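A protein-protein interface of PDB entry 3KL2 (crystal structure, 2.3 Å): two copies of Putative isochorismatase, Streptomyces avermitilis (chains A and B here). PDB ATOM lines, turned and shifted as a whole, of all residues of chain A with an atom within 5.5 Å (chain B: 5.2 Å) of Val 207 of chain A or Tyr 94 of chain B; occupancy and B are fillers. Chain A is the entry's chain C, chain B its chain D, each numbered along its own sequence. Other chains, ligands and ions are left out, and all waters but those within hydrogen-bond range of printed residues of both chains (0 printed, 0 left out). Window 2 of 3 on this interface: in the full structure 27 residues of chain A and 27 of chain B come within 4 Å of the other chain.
The side-chain hydroxyl (OH) of Tyr 94 of chain B sits at hydrogen-bond distance from the backbone carbonyl oxygen (O) of Phe 177 of chain A (2.9 Å). The backbone NH of Ile 96 of chain B lies within hydrogen-bond range of the backbone carbonyl oxygen of Met 204 of chain A (2.8 Å). OH of Tyr 173 of chain A sits close to O of Tyr 94 of chain B (2.4 Å). OH of Tyr 173 of chain A lies within hydrogen-bond range of N of Ile 96 of chain B (3.4 Å). The backbone NH of Val 179 of chain A sits at hydrogen-bond distance from the side-chain hydroxyl of Tyr 94 of chain B, at 3.0 Å. The side-chain hydroxyl (OH) of Tyr 173 of chain A is in hydrogen-bond range of the backbone NH (N) of Leu 97 of chain B (3.3 Å).
The backbone carbonyl oxygen (O) of Val 179 of chain A sits at hydrogen-bond distance from the backbone NH (N) of Val 207 of chain A (2.9 Å). The backbone carbonyl oxygen of Val 207 of chain A sits at hydrogen-bond distance from the backbone NH of Thr 181 of chain A (3.3 Å). The side-chain hydroxyl (OG1) of Thr 181 of chain A lies within hydrogen-bond range of the side-chain hydroxyl (OG) of Ser 206 of chain A (3.0 Å). O of Phe 202 of chain A lies within hydrogen-bond range of OG of Ser 206 of chain A, 2.5 Å away.
Among the printed residues, merely in contact across the chains: Tyr 173 of chain A with Gly 95 of chain B (3.6 Å), Arg 178 of chain A with Tyr 94 of chain B (3.6 Å), Met 204 of chain A with Gly 95 of chain B (3.2 Å), Phe 205 of chain A with Tyr 94 of chain B (3.8 Å), Ser 206 of chain A with Tyr 94 of chain B (3.6 Å) and Val 207 of chain A with Tyr 94 of chain B (3.9 Å).
Printed residues of chain B within 4 Å of Val 207 of chain A: Tyr 94 (3.9 Å). Tyr 94 of chain B touches just these residues of chain A: Tyr 173, Phe 177, Arg 178, Val 179, Phe 205, Ser 206 and Val 207. Printed residues of chain A within 4 Å of Leu 97 of chain B: Tyr 173. Of the printed residues of chain B, Phe 177 of chain A touches Tyr 94 (2.9 Å). Of the printed residues of chain B, Ser 206 of chain A touches Tyr 94. Of the printed residues of chain A, Ile 96 of chain B touches Tyr 173 (3.4 Å) and Met 204 (2.8 Å). Printed residues of chain A within 4 Å of Gly 95 of chain B: Tyr 173 and Met 204. Phe 202 of chain A touches none of the printed residues of chain B. His 92 of chain B touches none of the printed residues of chain A. The nearest printed residue of chain B that does not touch Val 207 of chain A is Gly 95 of chain B (6.4 Å). The nearest residue of chain A that does not touch Tyr 94 of chain B is Met 204 of chain A (4.8 Å).
Of the 7 printed residues of chain B, 4 touch a printed residue of chain A. Hydrophobic or aromatic side chains of chain B within 4 Å of the printed part of chain A: Tyr 94, Ile 96 and Leu 97. Of the 13 printed residues of chain A, 8 touch a printed residue of chain B. Hydrophobic or aromatic side chains of chain A that line the printed part of chain B: Tyr 173, Val 179 and Val 207. Along chain A the printed residues that touch a printed residue of chain B span positions 173 to 207. Among the printed residues, 12 pairs touch across the chains. Among the printed residues, no Asp or Glu carboxylate lies within 4 Å of a Lys or Arg side-chain nitrogen of the other chain.
No position is printed for both chains.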
ATOM      1  N   TYR A 173     -10.078  -8.638  20.542  1.00  0.00           N
ATOM      2  CA  TYR A 173     -10.655  -7.334  20.262  1.00  0.00           C
ATOM      3  C   TYR A 173     -10.655  -7.023  18.768  1.00  0.00           C
ATOM      4  O   TYR A 173     -11.690  -6.638  18.228  1.00  0.00           O
ATOM      5  CB  TYR A 173      -9.891  -6.255  21.031  1.00  0.00           C
ATOM      6  CG  TYR A 173     -10.532  -4.881  21.036  1.00  0.00           C
ATOM      7  CD1 TYR A 173     -11.634  -4.628  21.797  1.00  0.00           C
ATOM      8  CD2 TYR A 173     -10.009  -3.846  20.297  1.00  0.00           C
ATOM      9  CE1 TYR A 173     -12.220  -3.383  21.829  1.00  0.00           C
ATOM     10  CE2 TYR A 173     -10.602  -2.593  20.294  1.00  0.00           C
ATOM     11  CZ  TYR A 173     -11.728  -2.365  21.072  1.00  0.00           C
ATOM     12  OH  TYR A 173     -12.346  -1.107  21.141  1.00  0.00           O
ATOM     13  N   PHE A 177     -14.579  -9.993  18.840  1.00  0.00           N
ATOM     14  CA  PHE A 177     -15.103 -10.718  19.979  1.00  0.00           C
ATOM     15  C   PHE A 177     -15.428  -9.748  21.120  1.00  0.00           C
ATOM     16  O   PHE A 177     -14.827  -8.699  21.212  1.00  0.00           O
ATOM     17  CB  PHE A 177     -14.095 -11.773  20.454  1.00  0.00           C
ATOM     18  CG  PHE A 177     -13.952 -12.963  19.534  1.00  0.00           C
ATOM     19  CD1 PHE A 177     -14.929 -13.948  19.482  1.00  0.00           C
ATOM     20  CD2 PHE A 177     -12.852 -13.101  18.747  1.00  0.00           C
ATOM     21  CE1 PHE A 177     -14.778 -15.029  18.688  1.00  0.00           C
ATOM     22  CE2 PHE A 177     -12.697 -14.161  17.950  1.00  0.00           C
ATOM     23  CZ  PHE A 177     -13.644 -15.134  17.899  1.00  0.00           C
ATOM     24  N   ARG A 178     -16.413 -10.068  21.944  1.00  0.00           N
ATOM     25  CA  ARG A 178     -16.585  -9.361  23.176  1.00  0.00           C
ATOM     26  C   ARG A 178     -15.698 -10.100  24.195  1.00  0.00           C
ATOM     27  O   ARG A 178     -15.955 -11.257  24.507  1.00  0.00           O
ATOM     28  CB  ARG A 178     -18.039  -9.369  23.621  1.00  0.00           C
ATOM     29  CG  ARG A 178     -18.220  -8.660  24.983  1.00  0.00           C
ATOM     30  CD  ARG A 178     -19.653  -8.477  25.405  1.00  0.00           C
ATOM     31  NE  ARG A 178     -20.324  -9.767  25.565  1.00  0.00           N
ATOM     32  CZ  ARG A 178     -21.452  -9.958  26.234  1.00  0.00           C
ATOM     33  NH1 ARG A 178     -22.062  -8.955  26.843  1.00  0.00           N
ATOM     34  NH2 ARG A 178     -21.950 -11.168  26.305  1.00  0.00           N
ATOM     35  N   VAL A 179     -14.628  -9.442  24.653  1.00  0.00           N
ATOM     36  CA  VAL A 179     -13.583 -10.083  25.431  1.00  0.00           C
ATOM     37  C   VAL A 179     -13.781  -9.634  26.851  1.00  0.00           C
ATOM     38  O   VAL A 179     -13.787  -8.446  27.104  1.00  0.00           O
ATOM     39  CB  VAL A 179     -12.161  -9.648  24.965  1.00  0.00           C
ATOM     40  CG1 VAL A 179     -11.111 -10.208  25.903  1.00  0.00           C
ATOM     41  CG2 VAL A 179     -11.887 -10.092  23.551  1.00  0.00           C
ATOM     42  N   ILE A 180     -14.021 -10.578  27.761  1.00  0.00           N
ATOM     43  CA  ILE A 180     -14.067 -10.323  29.183  1.00  0.00           C
ATOM     44  C   ILE A 180     -12.774 -10.876  29.771  1.00  0.00           C
ATOM     45  O   ILE A 180     -12.408 -12.026  29.528  1.00  0.00           O
ATOM     46  CB  ILE A 180     -15.280 -10.992  29.821  1.00  0.00           C
ATOM     47  CG1 ILE A 180     -16.592 -10.253  29.404  1.00  0.00           C
ATOM     48  CG2 ILE A 180     -15.158 -10.969  31.325  1.00  0.00           C
ATOM     49  CD1 ILE A 180     -17.818 -11.183  29.176  1.00  0.00           C
ATOM     50  N   THR A 181     -12.057 -10.013  30.491  1.00  0.00           N
ATOM     51  CA  THR A 181     -10.877 -10.389  31.223  1.00  0.00           C
ATOM     52  C   THR A 181     -11.247 -10.513  32.717  1.00  0.00           C
ATOM     53  O   THR A 181     -11.854  -9.594  33.335  1.00  0.00           O
ATOM     54  CB  THR A 181      -9.743  -9.376  31.004  1.00  0.00           C
ATOM     55  OG1 THR A 181     -10.220  -8.055  31.268  1.00  0.00           O
ATOM     56  CG2 THR A 181      -9.204  -9.461  29.540  1.00  0.00           C
ATOM     57  N   PHE A 202      -6.046  -3.439  30.000  1.00  0.00           N
ATOM     58  CA  PHE A 202      -7.241  -4.263  29.927  1.00  0.00           C
ATOM     59  C   PHE A 202      -8.478  -3.478  29.468  1.00  0.00           C
ATOM     60  O   PHE A 202      -9.201  -3.926  28.571  1.00  0.00           O
ATOM     61  CB  PHE A 202      -7.495  -5.017  31.232  1.00  0.00           C
ATOM     62  CG  PHE A 202      -6.724  -6.308  31.368  1.00  0.00           C
ATOM     63  CD1 PHE A 202      -7.238  -7.353  32.113  1.00  0.00           C
ATOM     64  CD2 PHE A 202      -5.485  -6.479  30.781  1.00  0.00           C
ATOM     65  CE1 PHE A 202      -6.527  -8.517  32.254  1.00  0.00           C
ATOM     66  CE2 PHE A 202      -4.789  -7.662  30.897  1.00  0.00           C
ATOM     67  CZ  PHE A 202      -5.304  -8.665  31.610  1.00  0.00           C
ATOM     68  N   MET A 204      -8.702  -0.990  27.540  1.00  0.00           N
ATOM     69  CA  MET A 204      -8.608  -0.664  26.109  1.00  0.00           C
ATOM     70  C   MET A 204      -9.216  -1.747  25.260  1.00  0.00           C
ATOM     71  O   MET A 204      -9.865  -1.439  24.273  1.00  0.00           O
ATOM     72  CB  MET A 204      -7.147  -0.444  25.653  1.00  0.00           C
ATOM     73  CG  MET A 204      -6.487   0.912  26.093  1.00  0.00           C
ATOM     74  SD  MET A 204      -4.686   0.953  25.729  1.00  0.00           S
ATOM     75  CE  MET A 204      -4.538   2.630  25.231  1.00  0.00           C
ATOM     76  N   PHE A 205      -8.988  -3.015  25.607  1.00  0.00           N
ATOM     77  CA  PHE A 205      -9.350  -4.145  24.721  1.00  0.00           C
ATOM     78  C   PHE A 205     -10.337  -5.134  25.284  1.00  0.00           C
ATOM     79  O   PHE A 205     -10.570  -6.174  24.661  1.00  0.00           O
ATOM     80  CB  PHE A 205      -8.138  -4.934  24.304  1.00  0.00           C
ATOM     81  CG  PHE A 205      -7.017  -4.101  23.687  1.00  0.00           C
ATOM     82  CD1 PHE A 205      -6.934  -3.921  22.320  1.00  0.00           C
ATOM     83  CD2 PHE A 205      -6.060  -3.512  24.477  1.00  0.00           C
ATOM     84  CE1 PHE A 205      -5.893  -3.177  21.746  1.00  0.00           C
ATOM     85  CE2 PHE A 205      -5.031  -2.773  23.917  1.00  0.00           C
ATOM     86  CZ  PHE A 205      -4.940  -2.614  22.537  1.00  0.00           C
ATOM     87  N   SER A 206     -10.935  -4.831  26.439  1.00  0.00           N
ATOM     88  CA  SER A 206     -11.789  -5.799  27.075  1.00  0.00           C
ATOM     89  C   SER A 206     -12.719  -5.136  28.020  1.00  0.00           C
ATOM     90  O   SER A 206     -12.607  -3.943  28.280  1.00  0.00           O
ATOM     91  CB  SER A 206     -10.935  -6.816  27.848  1.00  0.00           C
ATOM     92  OG  SER A 206     -10.214  -6.205  28.954  1.00  0.00           O
ATOM     93  N   VAL A 207     -13.642  -5.942  28.540  1.00  0.00           N
ATOM     94  CA  VAL A 207     -14.509  -5.579  29.665  1.00  0.00           C
ATOM     95  C   VAL A 207     -13.979  -6.346  30.874  1.00  0.00           C
ATOM     96  O   VAL A 207     -14.168  -7.556  30.957  1.00  0.00           O
ATOM     97  CB  VAL A 207     -15.986  -5.934  29.396  1.00  0.00           C
ATOM     98  CG1 VAL A 207     -16.884  -5.494  30.561  1.00  0.00           C
ATOM     99  CG2 VAL A 207     -16.474  -5.236  28.116  1.00  0.00           C
ATOM    100  N   PRO A 208     -13.284  -5.651  31.787  1.00  0.00           N
ATOM    101  CA  PRO A 208     -12.654  -6.295  32.934  1.00  0.00           C
ATOM    102  C   PRO A 208     -13.643  -6.646  34.034  1.00  0.00           C
ATOM    103  O   PRO A 208     -14.490  -5.829  34.449  1.00  0.00           O
ATOM    104  CB  PRO A 208     -11.653  -5.251  33.430  1.00  0.00           C
ATOM    105  CG  PRO A 208     -11.577  -4.199  32.253  1.00  0.00           C
ATOM    106  CD  PRO A 208     -12.930  -4.219  31.702  1.00  0.00           C
ATOM    107  N   MET A 209     -13.571  -7.874  34.498  1.00  0.00           N
ATOM    108  CA  MET A 209     -14.542  -8.313  35.457  1.00  0.00           C
ATOM    109  C   MET A 209     -13.851  -9.163  36.499  1.00  0.00           C
ATOM    110  O   MET A 209     -12.846  -9.807  36.214  1.00  0.00           O
ATOM    111  CB  MET A 209     -15.638  -9.102  34.750  1.00  0.00           C
ATOM    112  CG  MET A 209     -16.381  -8.280  33.685  1.00  0.00           C
ATOM    113  SD  MET A 209     -18.139  -8.710  33.538  1.00  0.00           S
ATOM    114  CE  MET A 209     -18.101  -9.835  32.239  1.00  0.00           C
ATOM    115  N   HIS B  92     -22.108   0.304  18.569  1.00  0.00           N
ATOM    116  CA  HIS B  92     -21.887   0.278  20.021  1.00  0.00           C
ATOM    117  C   HIS B  92     -20.452  -0.214  20.390  1.00  0.00           C
ATOM    118  O   HIS B  92     -20.274  -1.259  21.007  1.00  0.00           O
ATOM    119  CB  HIS B  92     -22.928  -0.655  20.624  1.00  0.00           C
ATOM    120  CG  HIS B  92     -24.346  -0.243  20.355  1.00  0.00           C
ATOM    121  ND1 HIS B  92     -24.768   1.069  20.428  1.00  0.00           N
ATOM    122  CD2 HIS B  92     -25.446  -0.975  20.049  1.00  0.00           C
ATOM    123  CE1 HIS B  92     -26.065   1.128  20.170  1.00  0.00           C
ATOM    124  NE2 HIS B  92     -26.499  -0.099  19.927  1.00  0.00           N
ATOM    125  N   PRO B  93     -19.426   0.543  20.008  1.00  0.00           N
ATOM    126  CA  PRO B  93     -18.076   0.130  20.351  1.00  0.00           C
ATOM    127  C   PRO B  93     -17.796   0.137  21.875  1.00  0.00           C
ATOM    128  O   PRO B  93     -18.470   0.855  22.657  1.00  0.00           O
ATOM    129  CB  PRO B  93     -17.225   1.180  19.650  1.00  0.00           C
ATOM    130  CG  PRO B  93     -18.038   2.371  19.744  1.00  0.00           C
ATOM    131  CD  PRO B  93     -19.435   1.906  19.467  1.00  0.00           C
ATOM    132  N   TYR B  94     -16.820  -0.682  22.281  1.00  0.00           N
ATOM    133  CA  TYR B  94     -16.319  -0.662  23.662  1.00  0.00           C
ATOM    134  C   TYR B  94     -14.818  -0.555  23.587  1.00  0.00           C
ATOM    135  O   TYR B  94     -14.228  -0.681  22.501  1.00  0.00           O
ATOM    136  CB  TYR B  94     -16.811  -1.873  24.476  1.00  0.00           C
ATOM    137  CG  TYR B  94     -16.088  -3.184  24.172  1.00  0.00           C
ATOM    138  CD1 TYR B  94     -16.523  -4.022  23.146  1.00  0.00           C
ATOM    139  CD2 TYR B  94     -14.968  -3.583  24.921  1.00  0.00           C
ATOM    140  CE1 TYR B  94     -15.846  -5.225  22.839  1.00  0.00           C
ATOM    141  CE2 TYR B  94     -14.289  -4.772  24.638  1.00  0.00           C
ATOM    142  CZ  TYR B  94     -14.730  -5.605  23.596  1.00  0.00           C
ATOM    143  OH  TYR B  94     -14.071  -6.797  23.317  1.00  0.00           O
ATOM    144  N   GLY B  95     -14.189  -0.288  24.727  1.00  0.00           N
ATOM    145  CA  GLY B  95     -12.743  -0.158  24.770  1.00  0.00           C
ATOM    146  C   GLY B  95     -12.217   1.043  24.035  1.00  0.00           C
ATOM    147  O   GLY B  95     -12.881   2.046  23.933  1.00  0.00           O
ATOM    148  N   ILE B  96     -11.014   0.943  23.504  1.00  0.00           N
ATOM    149  CA  ILE B  96     -10.341   2.124  23.040  1.00  0.00           C
ATOM    150  C   ILE B  96     -11.028   2.835  21.822  1.00  0.00           C
ATOM    151  O   ILE B  96     -11.075   4.076  21.756  1.00  0.00           O
ATOM    152  CB  ILE B  96      -8.842   1.809  22.775  1.00  0.00           C
ATOM    153  CG1 ILE B  96      -8.066   3.108  22.495  1.00  0.00           C
ATOM    154  CG2 ILE B  96      -8.680   0.771  21.703  1.00  0.00           C
ATOM    155  CD1 ILE B  96      -8.244   4.146  23.626  1.00  0.00           C
ATOM    156  N   LEU B  97     -11.592   2.065  20.894  1.00  0.00           N
ATOM    157  CA  LEU B  97     -12.194   2.640  19.714  1.00  0.00           C
ATOM    158  C   LEU B  97     -13.445   3.431  20.082  1.00  0.00           C
ATOM    159  O   LEU B  97     -13.815   4.371  19.397  1.00  0.00           O
ATOM    160  CB  LEU B  97     -12.484   1.555  18.686  1.00  0.00           C
ATOM    161  CG  LEU B  97     -11.232   0.933  18.033  1.00  0.00           C
ATOM    162  CD1 LEU B  97     -11.587  -0.306  17.171  1.00  0.00           C
ATOM    163  CD2 LEU B  97     -10.487   1.973  17.192  1.00  0.00           C
ATOM    164  N   LYS B  98     -14.092   3.097  21.187  1.00  0.00           N
ATOM    165  CA  LYS B  98     -15.194   3.937  21.655  1.00  0.00           C
ATOM    166  C   LYS B  98     -14.792   5.407  21.743  1.00  0.00           C
ATOM    167  O   LYS B  98     -15.592   6.328  21.487  1.00  0.00           O
ATOM    168  CB  LYS B  98     -15.675   3.472  22.997  1.00  0.00           C
ATOM    169  CG  LYS B  98     -16.785   4.329  23.562  1.00  0.00           C
ATOM    170  CD  LYS B  98     -17.575   3.620  24.656  1.00  0.00           C
ATOM    171  CE  LYS B  98     -18.673   4.529  25.215  1.00  0.00           C
ATOM    172  NZ  LYS B  98     -18.224   5.962  25.119  1.00  0.00           N
